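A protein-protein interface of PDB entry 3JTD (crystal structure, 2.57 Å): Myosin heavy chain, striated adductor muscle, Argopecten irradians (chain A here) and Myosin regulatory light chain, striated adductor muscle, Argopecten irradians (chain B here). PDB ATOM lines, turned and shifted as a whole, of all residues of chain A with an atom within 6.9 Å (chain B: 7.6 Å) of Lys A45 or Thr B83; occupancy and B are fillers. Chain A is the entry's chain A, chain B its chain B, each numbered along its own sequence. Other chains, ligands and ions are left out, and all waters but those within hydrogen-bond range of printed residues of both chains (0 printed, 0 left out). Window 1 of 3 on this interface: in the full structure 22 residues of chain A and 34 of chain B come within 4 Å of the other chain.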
ATOM      1  N   GLN A  40      16.533  -2.049 -22.219  1.00  0.00           N
ATOM      2  CA  GLN A  40      17.472  -3.063 -21.754  1.00  0.00           C
ATOM      3  C   GLN A  40      18.849  -2.453 -21.430  1.00  0.00           C
ATOM      4  O   GLN A  40      19.441  -2.782 -20.394  1.00  0.00           O
ATOM      5  CB  GLN A  40      17.607  -4.193 -22.789  1.00  0.00           C
ATOM      6  CG  GLN A  40      16.340  -5.047 -22.922  1.00  0.00           C
ATOM      7  CD  GLN A  40      16.355  -6.013 -24.110  1.00  0.00           C
ATOM      8  OE1 GLN A  40      16.908  -5.706 -25.167  1.00  0.00           O
ATOM      9  NE2 GLN A  40      15.727  -7.183 -23.944  1.00  0.00           N
ATOM     10  N   ARG A  41      19.356  -1.566 -22.287  1.00  0.00           N
ATOM     11  CA  ARG A  41      20.655  -0.920 -22.050  1.00  0.00           C
ATOM     12  C   ARG A  41      20.708  -0.057 -20.778  1.00  0.00           C
ATOM     13  O   ARG A  41      21.677  -0.124 -20.026  1.00  0.00           O
ATOM     14  CB  ARG A  41      21.081  -0.066 -23.271  1.00  0.00           C
ATOM     15  CG  ARG A  41      22.292   0.883 -23.022  1.00  0.00           C
ATOM     16  CD  ARG A  41      22.999   1.377 -24.320  1.00  0.00           C
ATOM     17  NE  ARG A  41      22.078   1.987 -25.279  1.00  0.00           N
ATOM     18  CZ  ARG A  41      21.588   3.220 -25.196  1.00  0.00           C
ATOM     19  NH1 ARG A  41      20.735   3.641 -26.115  1.00  0.00           N
ATOM     20  NH2 ARG A  41      21.972   4.036 -24.221  1.00  0.00           N
ATOM     21  N   ASN A  42      19.683   0.747 -20.519  1.00  0.00           N
ATOM     22  CA  ASN A  42      19.705   1.608 -19.335  1.00  0.00           C
ATOM     23  C   ASN A  42      19.530   0.866 -17.995  1.00  0.00           C
ATOM     24  O   ASN A  42      20.191   1.189 -17.005  1.00  0.00           O
ATOM     25  CB  ASN A  42      18.675   2.731 -19.515  1.00  0.00           C
ATOM     26  CG  ASN A  42      19.128   3.774 -20.543  1.00  0.00           C
ATOM     27  OD1 ASN A  42      19.975   4.622 -20.250  1.00  0.00           O
ATOM     28  ND2 ASN A  42      18.584   3.698 -21.758  1.00  0.00           N
ATOM     29  N   ILE A  43      18.650  -0.140 -17.966  1.00  0.00           N
ATOM     30  CA  ILE A  43      18.456  -0.934 -16.756  1.00  0.00           C
ATOM     31  C   ILE A  43      19.802  -1.661 -16.492  1.00  0.00           C
ATOM     32  O   ILE A  43      20.228  -1.838 -15.337  1.00  0.00           O
ATOM     33  CB  ILE A  43      17.303  -1.981 -16.941  1.00  0.00           C
ATOM     34  CG1 ILE A  43      15.933  -1.264 -16.938  1.00  0.00           C
ATOM     35  CG2 ILE A  43      17.365  -3.042 -15.832  1.00  0.00           C
ATOM     36  CD1 ILE A  43      14.802  -2.103 -17.414  1.00  0.00           C
ATOM     37  N   ARG A  44      20.481  -2.053 -17.567  1.00  0.00           N
ATOM     38  CA  ARG A  44      21.759  -2.718 -17.398  1.00  0.00           C
ATOM     39  C   ARG A  44      22.819  -1.774 -16.824  1.00  0.00           C
ATOM     40  O   ARG A  44      23.645  -2.203 -16.002  1.00  0.00           O
ATOM     41  CB  ARG A  44      22.230  -3.348 -18.718  1.00  0.00           C
ATOM     42  CG  ARG A  44      21.641  -4.750 -18.955  1.00  0.00           C
ATOM     43  CD  ARG A  44      22.289  -5.476 -20.131  1.00  0.00           C
ATOM     44  NE  ARG A  44      21.941  -6.899 -20.179  1.00  0.00           N
ATOM     45  CZ  ARG A  44      21.177  -7.462 -21.116  1.00  0.00           C
ATOM     46  NH1 ARG A  44      20.916  -8.774 -21.080  1.00  0.00           N
ATOM     47  NH2 ARG A  44      20.653  -6.709 -22.081  1.00  0.00           N
ATOM     48  N   LYS A  45      22.785  -0.495 -17.179  1.00  0.00           N
ATOM     49  CA  LYS A  45      23.789   0.424 -16.645  1.00  0.00           C
ATOM     50  C   LYS A  45      23.508   0.609 -15.170  1.00  0.00           C
ATOM     51  O   LYS A  45      24.424   0.630 -14.340  1.00  0.00           O
ATOM     52  CB  LYS A  45      23.725   1.779 -17.357  1.00  0.00           C
ATOM     53  CG  LYS A  45      24.187   1.749 -18.809  1.00  0.00           C
ATOM     54  CD  LYS A  45      25.712   1.758 -18.917  1.00  0.00           C
ATOM     55  CE  LYS A  45      26.147   1.720 -20.388  1.00  0.00           C
ATOM     56  NZ  LYS A  45      27.626   1.711 -20.599  1.00  0.00           N
ATOM     57  N   TRP A  46      22.225   0.761 -14.853  1.00  0.00           N
ATOM     58  CA  TRP A  46      21.775   0.904 -13.469  1.00  0.00           C
ATOM     59  C   TRP A  46      22.270  -0.277 -12.601  1.00  0.00           C
ATOM     60  O   TRP A  46      22.825  -0.080 -11.518  1.00  0.00           O
ATOM     61  CB  TRP A  46      20.252   0.973 -13.465  1.00  0.00           C
ATOM     62  CG  TRP A  46      19.626   1.014 -12.126  1.00  0.00           C
ATOM     63  CD1 TRP A  46      19.722   2.010 -11.198  1.00  0.00           C
ATOM     64  CD2 TRP A  46      18.730   0.042 -11.585  1.00  0.00           C
ATOM     65  NE1 TRP A  46      18.930   1.720 -10.111  1.00  0.00           N
ATOM     66  CE2 TRP A  46      18.309   0.517 -10.324  1.00  0.00           C
ATOM     67  CE3 TRP A  46      18.240  -1.185 -12.048  1.00  0.00           C
ATOM     68  CZ2 TRP A  46      17.415  -0.193  -9.518  1.00  0.00           C
ATOM     69  CZ3 TRP A  46      17.349  -1.892 -11.245  1.00  0.00           C
ATOM     70  CH2 TRP A  46      16.945  -1.392  -9.994  1.00  0.00           C
ATOM     71  N   LEU A  47      22.096  -1.497 -13.102  1.00  0.00           N
ATOM     72  CA  LEU A  47      22.556  -2.652 -12.360  1.00  0.00           C
ATOM     73  C   LEU A  47      24.087  -2.584 -12.071  1.00  0.00           C
ATOM     74  O   LEU A  47      24.521  -2.718 -10.911  1.00  0.00           O
ATOM     75  CB  LEU A  47      22.185  -3.964 -13.093  1.00  0.00           C
ATOM     76  CG  LEU A  47      20.689  -4.337 -13.223  1.00  0.00           C
ATOM     77  CD1 LEU A  47      20.532  -5.651 -13.925  1.00  0.00           C
ATOM     78  CD2 LEU A  47      20.018  -4.410 -11.885  1.00  0.00           C
ATOM     79  N   VAL A  48      24.888  -2.352 -13.110  1.00  0.00           N
ATOM     80  CA  VAL A  48      26.344  -2.277 -12.973  1.00  0.00           C
ATOM     81  C   VAL A  48      26.814  -1.195 -12.001  1.00  0.00           C
ATOM     82  O   VAL A  48      27.731  -1.406 -11.194  1.00  0.00           O
ATOM     83  CB  VAL A  48      27.020  -2.037 -14.350  1.00  0.00           C
ATOM     84  CG1 VAL A  48      28.489  -1.685 -14.156  1.00  0.00           C
ATOM     85  CG2 VAL A  48      26.891  -3.296 -15.233  1.00  0.00           C
ATOM     86  N   LEU A  49      26.180  -0.029 -12.082  1.00  0.00           N
ATOM     87  CA  LEU A  49      26.514   1.086 -11.203  1.00  0.00           C
ATOM     88  C   LEU A  49      26.209   0.752  -9.747  1.00  0.00           C
ATOM     89  O   LEU A  49      26.900   1.211  -8.837  1.00  0.00           O
ATOM     90  CB  LEU A  49      25.753   2.345 -11.624  1.00  0.00           C
ATOM     91  CG  LEU A  49      25.869   3.551 -10.688  1.00  0.00           C
ATOM     92  CD1 LEU A  49      27.326   3.938 -10.488  1.00  0.00           C
ATOM     93  CD2 LEU A  49      25.066   4.726 -11.224  1.00  0.00           C
ATOM     94  N   ARG A  50      25.171  -0.050  -9.534  1.00  0.00           N
ATOM     95  CA  ARG A  50      24.745  -0.410  -8.187  1.00  0.00           C
ATOM     96  C   ARG A  50      25.732  -1.375  -7.537  1.00  0.00           C
ATOM     97  O   ARG A  50      25.781  -1.496  -6.312  1.00  0.00           O
ATOM     98  CB  ARG A  50      23.346  -1.030  -8.216  1.00  0.00           C
ATOM     99  CG  ARG A  50      22.219  -0.013  -8.288  1.00  0.00           C
ATOM    100  CD  ARG A  50      22.070   0.740  -6.977  1.00  0.00           C
ATOM    101  NE  ARG A  50      20.707   0.669  -6.455  1.00  0.00           N
ATOM    102  CZ  ARG A  50      20.360  -0.004  -5.364  1.00  0.00           C
ATOM    103  NH1 ARG A  50      19.095  -0.014  -4.965  1.00  0.00           N
ATOM    104  NH2 ARG A  50      21.275  -0.668  -4.671  1.00  0.00           N
ATOM    105  N   ASN A  51      26.516  -2.058  -8.364  1.00  0.00           N
ATOM    106  CA  ASN A  51      27.461  -3.054  -7.875  1.00  0.00           C
ATOM    107  C   ASN A  51      28.859  -2.476  -7.679  1.00  0.00           C
ATOM    108  O   ASN A  51      29.796  -3.196  -7.336  1.00  0.00           O
ATOM    109  CB  ASN A  51      27.516  -4.253  -8.825  1.00  0.00           C
ATOM    110  CG  ASN A  51      27.414  -5.579  -8.098  1.00  0.00           C
ATOM    111  OD1 ASN A  51      26.328  -6.142  -7.959  1.00  0.00           O
ATOM    112  ND2 ASN A  51      28.548  -6.085  -7.627  1.00  0.00           N
ATOM    113  N   LEU B  12      27.962  16.542 -17.360  1.00  0.00           N
ATOM    114  CA  LEU B  12      27.219  16.281 -16.166  1.00  0.00           C
ATOM    115  C   LEU B  12      27.453  17.408 -15.231  1.00  0.00           C
ATOM    116  O   LEU B  12      28.560  17.833 -14.943  1.00  0.00           O
ATOM    117  CB  LEU B  12      27.532  14.892 -15.640  1.00  0.00           C
ATOM    118  CG  LEU B  12      26.645  13.882 -16.333  1.00  0.00           C
ATOM    119  CD1 LEU B  12      26.380  12.710 -15.408  1.00  0.00           C
ATOM    120  CD2 LEU B  12      25.340  14.529 -16.783  1.00  0.00           C
ATOM    121  N   SER B  77      32.744   9.475 -14.301  1.00  0.00           N
ATOM    122  CA  SER B  77      32.194   9.833 -15.602  1.00  0.00           C
ATOM    123  C   SER B  77      32.202   8.669 -16.581  1.00  0.00           C
ATOM    124  O   SER B  77      31.303   8.566 -17.425  1.00  0.00           O
ATOM    125  CB  SER B  77      32.959  11.006 -16.210  1.00  0.00           C
ATOM    126  OG  SER B  77      32.657  12.209 -15.538  1.00  0.00           O
ATOM    127  N   ASP B  78      33.198   7.792 -16.472  1.00  0.00           N
ATOM    128  CA  ASP B  78      33.284   6.649 -17.381  1.00  0.00           C
ATOM    129  C   ASP B  78      32.128   5.719 -17.115  1.00  0.00           C
ATOM    130  O   ASP B  78      31.628   5.036 -18.012  1.00  0.00           O
ATOM    131  CB  ASP B  78      34.586   5.885 -17.170  1.00  0.00           C
ATOM    132  CG  ASP B  78      35.821   6.767 -17.332  1.00  0.00           C
ATOM    133  OD1 ASP B  78      36.895   6.363 -16.845  1.00  0.00           O
ATOM    134  OD2 ASP B  78      35.733   7.856 -17.942  1.00  0.00           O
ATOM    135  N   LYS B  79      31.695   5.715 -15.863  1.00  0.00           N
ATOM    136  CA  LYS B  79      30.612   4.857 -15.445  1.00  0.00           C
ATOM    137  C   LYS B  79      29.254   5.316 -15.946  1.00  0.00           C
ATOM    138  O   LYS B  79      28.358   4.504 -16.141  1.00  0.00           O
ATOM    139  CB  LYS B  79      30.605   4.756 -13.924  1.00  0.00           C
ATOM    140  CG  LYS B  79      30.546   3.336 -13.429  1.00  0.00           C
ATOM    141  CD  LYS B  79      31.745   2.573 -13.898  1.00  0.00           C
ATOM    142  CE  LYS B  79      31.808   1.219 -13.238  1.00  0.00           C
ATOM    143  NZ  LYS B  79      33.106   0.587 -13.528  1.00  0.00           N
ATOM    144  N   LEU B  80      29.107   6.621 -16.156  1.00  0.00           N
ATOM    145  CA  LEU B  80      27.840   7.193 -16.639  1.00  0.00           C
ATOM    146  C   LEU B  80      27.815   7.293 -18.165  1.00  0.00           C
ATOM    147  O   LEU B  80      26.971   7.969 -18.734  1.00  0.00           O
ATOM    148  CB  LEU B  80      27.613   8.575 -16.016  1.00  0.00           C
ATOM    149  CG  LEU B  80      27.316   8.551 -14.508  1.00  0.00           C
ATOM    150  CD1 LEU B  80      28.265   7.602 -13.822  1.00  0.00           C
ATOM    151  CD2 LEU B  80      27.464   9.921 -13.890  1.00  0.00           C
ATOM    152  N   SER B  81      28.759   6.625 -18.808  1.00  0.00           N
ATOM    153  CA  SER B  81      28.894   6.691 -20.252  1.00  0.00           C
ATOM    154  C   SER B  81      27.938   5.696 -20.902  1.00  0.00           C
ATOM    155  O   SER B  81      28.059   4.492 -20.705  1.00  0.00           O
ATOM    156  CB  SER B  81      30.342   6.388 -20.648  1.00  0.00           C
ATOM    157  OG  SER B  81      30.502   6.342 -22.051  1.00  0.00           O
ATOM    158  N   GLY B  82      26.979   6.206 -21.665  1.00  0.00           N
ATOM    159  CA  GLY B  82      26.066   5.351 -22.399  1.00  0.00           C
ATOM    160  C   GLY B  82      24.650   5.378 -21.863  1.00  0.00           C
ATOM    161  O   GLY B  82      23.889   4.436 -22.061  1.00  0.00           O
ATOM    162  N   THR B  83      24.296   6.467 -21.188  1.00  0.00           N
ATOM    163  CA  THR B  83      23.011   6.581 -20.515  1.00  0.00           C
ATOM    164  C   THR B  83      22.087   7.686 -21.035  1.00  0.00           C
ATOM    165  O   THR B  83      22.518   8.795 -21.289  1.00  0.00           O
ATOM    166  CB  THR B  83      23.237   6.761 -18.998  1.00  0.00           C
ATOM    167  OG1 THR B  83      23.880   8.015 -18.745  1.00  0.00           O
ATOM    168  CG2 THR B  83      24.132   5.637 -18.480  1.00  0.00           C
ATOM    169  N   ASP B  84      20.804   7.370 -21.154  1.00  0.00           N
ATOM    170  CA  ASP B  84      19.824   8.312 -21.672  1.00  0.00           C
ATOM    171  C   ASP B  84      19.143   9.057 -20.533  1.00  0.00           C
ATOM    172  O   ASP B  84      19.368   8.751 -19.368  1.00  0.00           O
ATOM    173  CB  ASP B  84      18.786   7.585 -22.524  1.00  0.00           C
ATOM    174  CG  ASP B  84      19.401   6.882 -23.716  1.00  0.00           C
ATOM    175  OD1 ASP B  84      19.610   5.656 -23.651  1.00  0.00           O
ATOM    176  OD2 ASP B  84      19.677   7.558 -24.725  1.00  0.00           O
ATOM    177  N   SER B  85      18.314  10.036 -20.875  1.00  0.00           N
ATOM    178  CA  SER B  85      17.597  10.821 -19.864  1.00  0.00           C
ATOM    179  C   SER B  85      16.218  10.216 -19.487  1.00  0.00           C
ATOM    180  O   SER B  85      15.746   9.254 -20.104  1.00  0.00           O
ATOM    181  CB  SER B  85      17.359  12.233 -20.381  1.00  0.00           C
ATOM    182  OG  SER B  85      16.325  12.203 -21.352  1.00  0.00           O
ATOM    183  N   THR B  88      13.540  10.429 -22.436  1.00  0.00           N
ATOM    184  CA  THR B  88      13.835   9.425 -23.457  1.00  0.00           C
ATOM    185  C   THR B  88      13.437   8.020 -22.969  1.00  0.00           C
ATOM    186  O   THR B  88      12.857   7.229 -23.741  1.00  0.00           O
ATOM    187  CB  THR B  88      15.356   9.395 -23.825  1.00  0.00           C
ATOM    188  OG1 THR B  88      15.755  10.663 -24.322  1.00  0.00           O
ATOM    189  CG2 THR B  88      15.670   8.329 -24.865  1.00  0.00           C
ATOM    190  N   ILE B  89      13.747   7.710 -21.707  1.00  0.00           N
ATOM    191  CA  ILE B  89      13.416   6.386 -21.152  1.00  0.00           C
ATOM    192  C   ILE B  89      11.889   6.194 -20.963  1.00  0.00           C
ATOM    193  O   ILE B  89      11.318   5.172 -21.363  1.00  0.00           O
ATOM    194  CB  ILE B  89      14.212   6.113 -19.825  1.00  0.00           C
ATOM    195  CG1 ILE B  89      15.715   6.054 -20.141  1.00  0.00           C
ATOM    196  CG2 ILE B  89      13.834   4.753 -19.265  1.00  0.00           C
ATOM    197  CD1 ILE B  89      16.641   6.096 -18.956  1.00  0.00           C
ATOM    198  N   ILE B 148      15.209   4.717 -11.108  1.00  0.00           N
ATOM    199  CA  ILE B 148      16.530   4.366 -11.610  1.00  0.00           C
ATOM    200  C   ILE B 148      17.312   5.574 -12.113  1.00  0.00           C
ATOM    201  O   ILE B 148      18.496   5.463 -12.390  1.00  0.00           O
ATOM    202  CB  ILE B 148      16.463   3.375 -12.767  1.00  0.00           C
ATOM    203  CG1 ILE B 148      15.994   4.113 -14.037  1.00  0.00           C
ATOM    204  CG2 ILE B 148      15.593   2.173 -12.358  1.00  0.00           C
ATOM    205  CD1 ILE B 148      15.957   3.240 -15.309  1.00  0.00           C
ATOM    206  N   LYS B 149      16.649   6.719 -12.252  1.00  0.00           N
ATOM    207  CA  LYS B 149      17.326   7.921 -12.724  1.00  0.00           C
ATOM    208  C   LYS B 149      17.808   8.696 -11.505  1.00  0.00           C
ATOM    209  O   LYS B 149      18.458   9.727 -11.616  1.00  0.00           O
ATOM    210  CB  LYS B 149      16.364   8.780 -13.555  1.00  0.00           C
ATOM    211  CG  LYS B 149      16.987   9.409 -14.785  1.00  0.00           C
ATOM    212  CD  LYS B 149      17.502   8.356 -15.734  1.00  0.00           C
ATOM    213  CE  LYS B 149      19.020   8.281 -15.706  1.00  0.00           C
ATOM    214  NZ  LYS B 149      19.676   9.108 -16.748  1.00  0.00           N
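Lys A45 touches just these residues of chain B: Ser B81, Gly B82 and Thr B83.
Thr B83 touches just these residues of chain A: Asn A42 (3.6 Å) and Lys A45 (3.9 Å).
Gly B82 touches just these residues of chain A: Arg A41 (2.9 Å) and Lys A45 (3.9 Å).
Printed residues of chain A within 4 Å of Ile B148: Trp A46.
Of the printed residues of chain A, Ser B81 touches Lys A45.
Of the printed residues of chain B, Asn A42 touches Thr B83, Asp B84 and Ile B89.
Of the printed residues of chain B, Arg A41 touches Gly B82 (2.9 Å) and Asp B84 (2.9 Å).
Printed residues of chain B within 4 Å of Trp A46: Ile B148 (3.8 Å).
The nearest residue of chain A that does not touch Thr B83 is Arg A41 (4.5 Å).
The nearest printed residue of chain B that does not touch Trp A46 is Lys B149 (5.7 Å).
O of Gly B82 is in hydrogen-bond range of NH2 of Arg A41 (2.9 Å).
The backbone carbonyl oxygen (O) of Ser B81 is in hydrogen-bond range of the side-chain amino group (NZ) of Lys A45.
NH2 of Arg A41 lies within salt-bridge range of OD1 of Asp B84 (2.9 Å).
The side-chain amide nitrogen (ND2) of Asn A42 is in hydrogen-bond range of the side-chain carboxylate (OD1) of Asp B84 (2.9 Å).
NZ of Lys B149 lies within hydrogen-bond range of O of Asp B84 (2.7 Å).
O of Leu B80 is in hydrogen-bond range of OG1 of Thr B83.
Of the 14 printed residues of chain B, 6 touch a printed residue of chain A.
Hydrophobic or aromatic side chains of chain B within 4 Å of the printed part of chain A: Ile B89 and Ile B148.
Of the 12 printed residues of chain A, 4 touch a printed residue of chain B.
Hydrophobic or aromatic side chains of chain A that line the printed part of chain B: Trp A46.
Among the printed residues, 9 pairs touch across the chains.
Among the printed residues, Asp or Glu carboxylates within 4 Å of a Lys or Arg side-chain nitrogen of the other chain: Arg A41 with Asp B84 (2.9 Å).
Asn A42 touches Thr B83 (OD1 to CA, 3.6 Å).
Ile B89 touches Asn A42 (CD1 to CG, 3.8 Å).
Gly B82 touches Lys A45 (O to CE, 3.9 Å).
Thr B83 touches Lys A45.
Trp A46 touches Ile B148 (CE2 to CG2, 3.8 Å).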
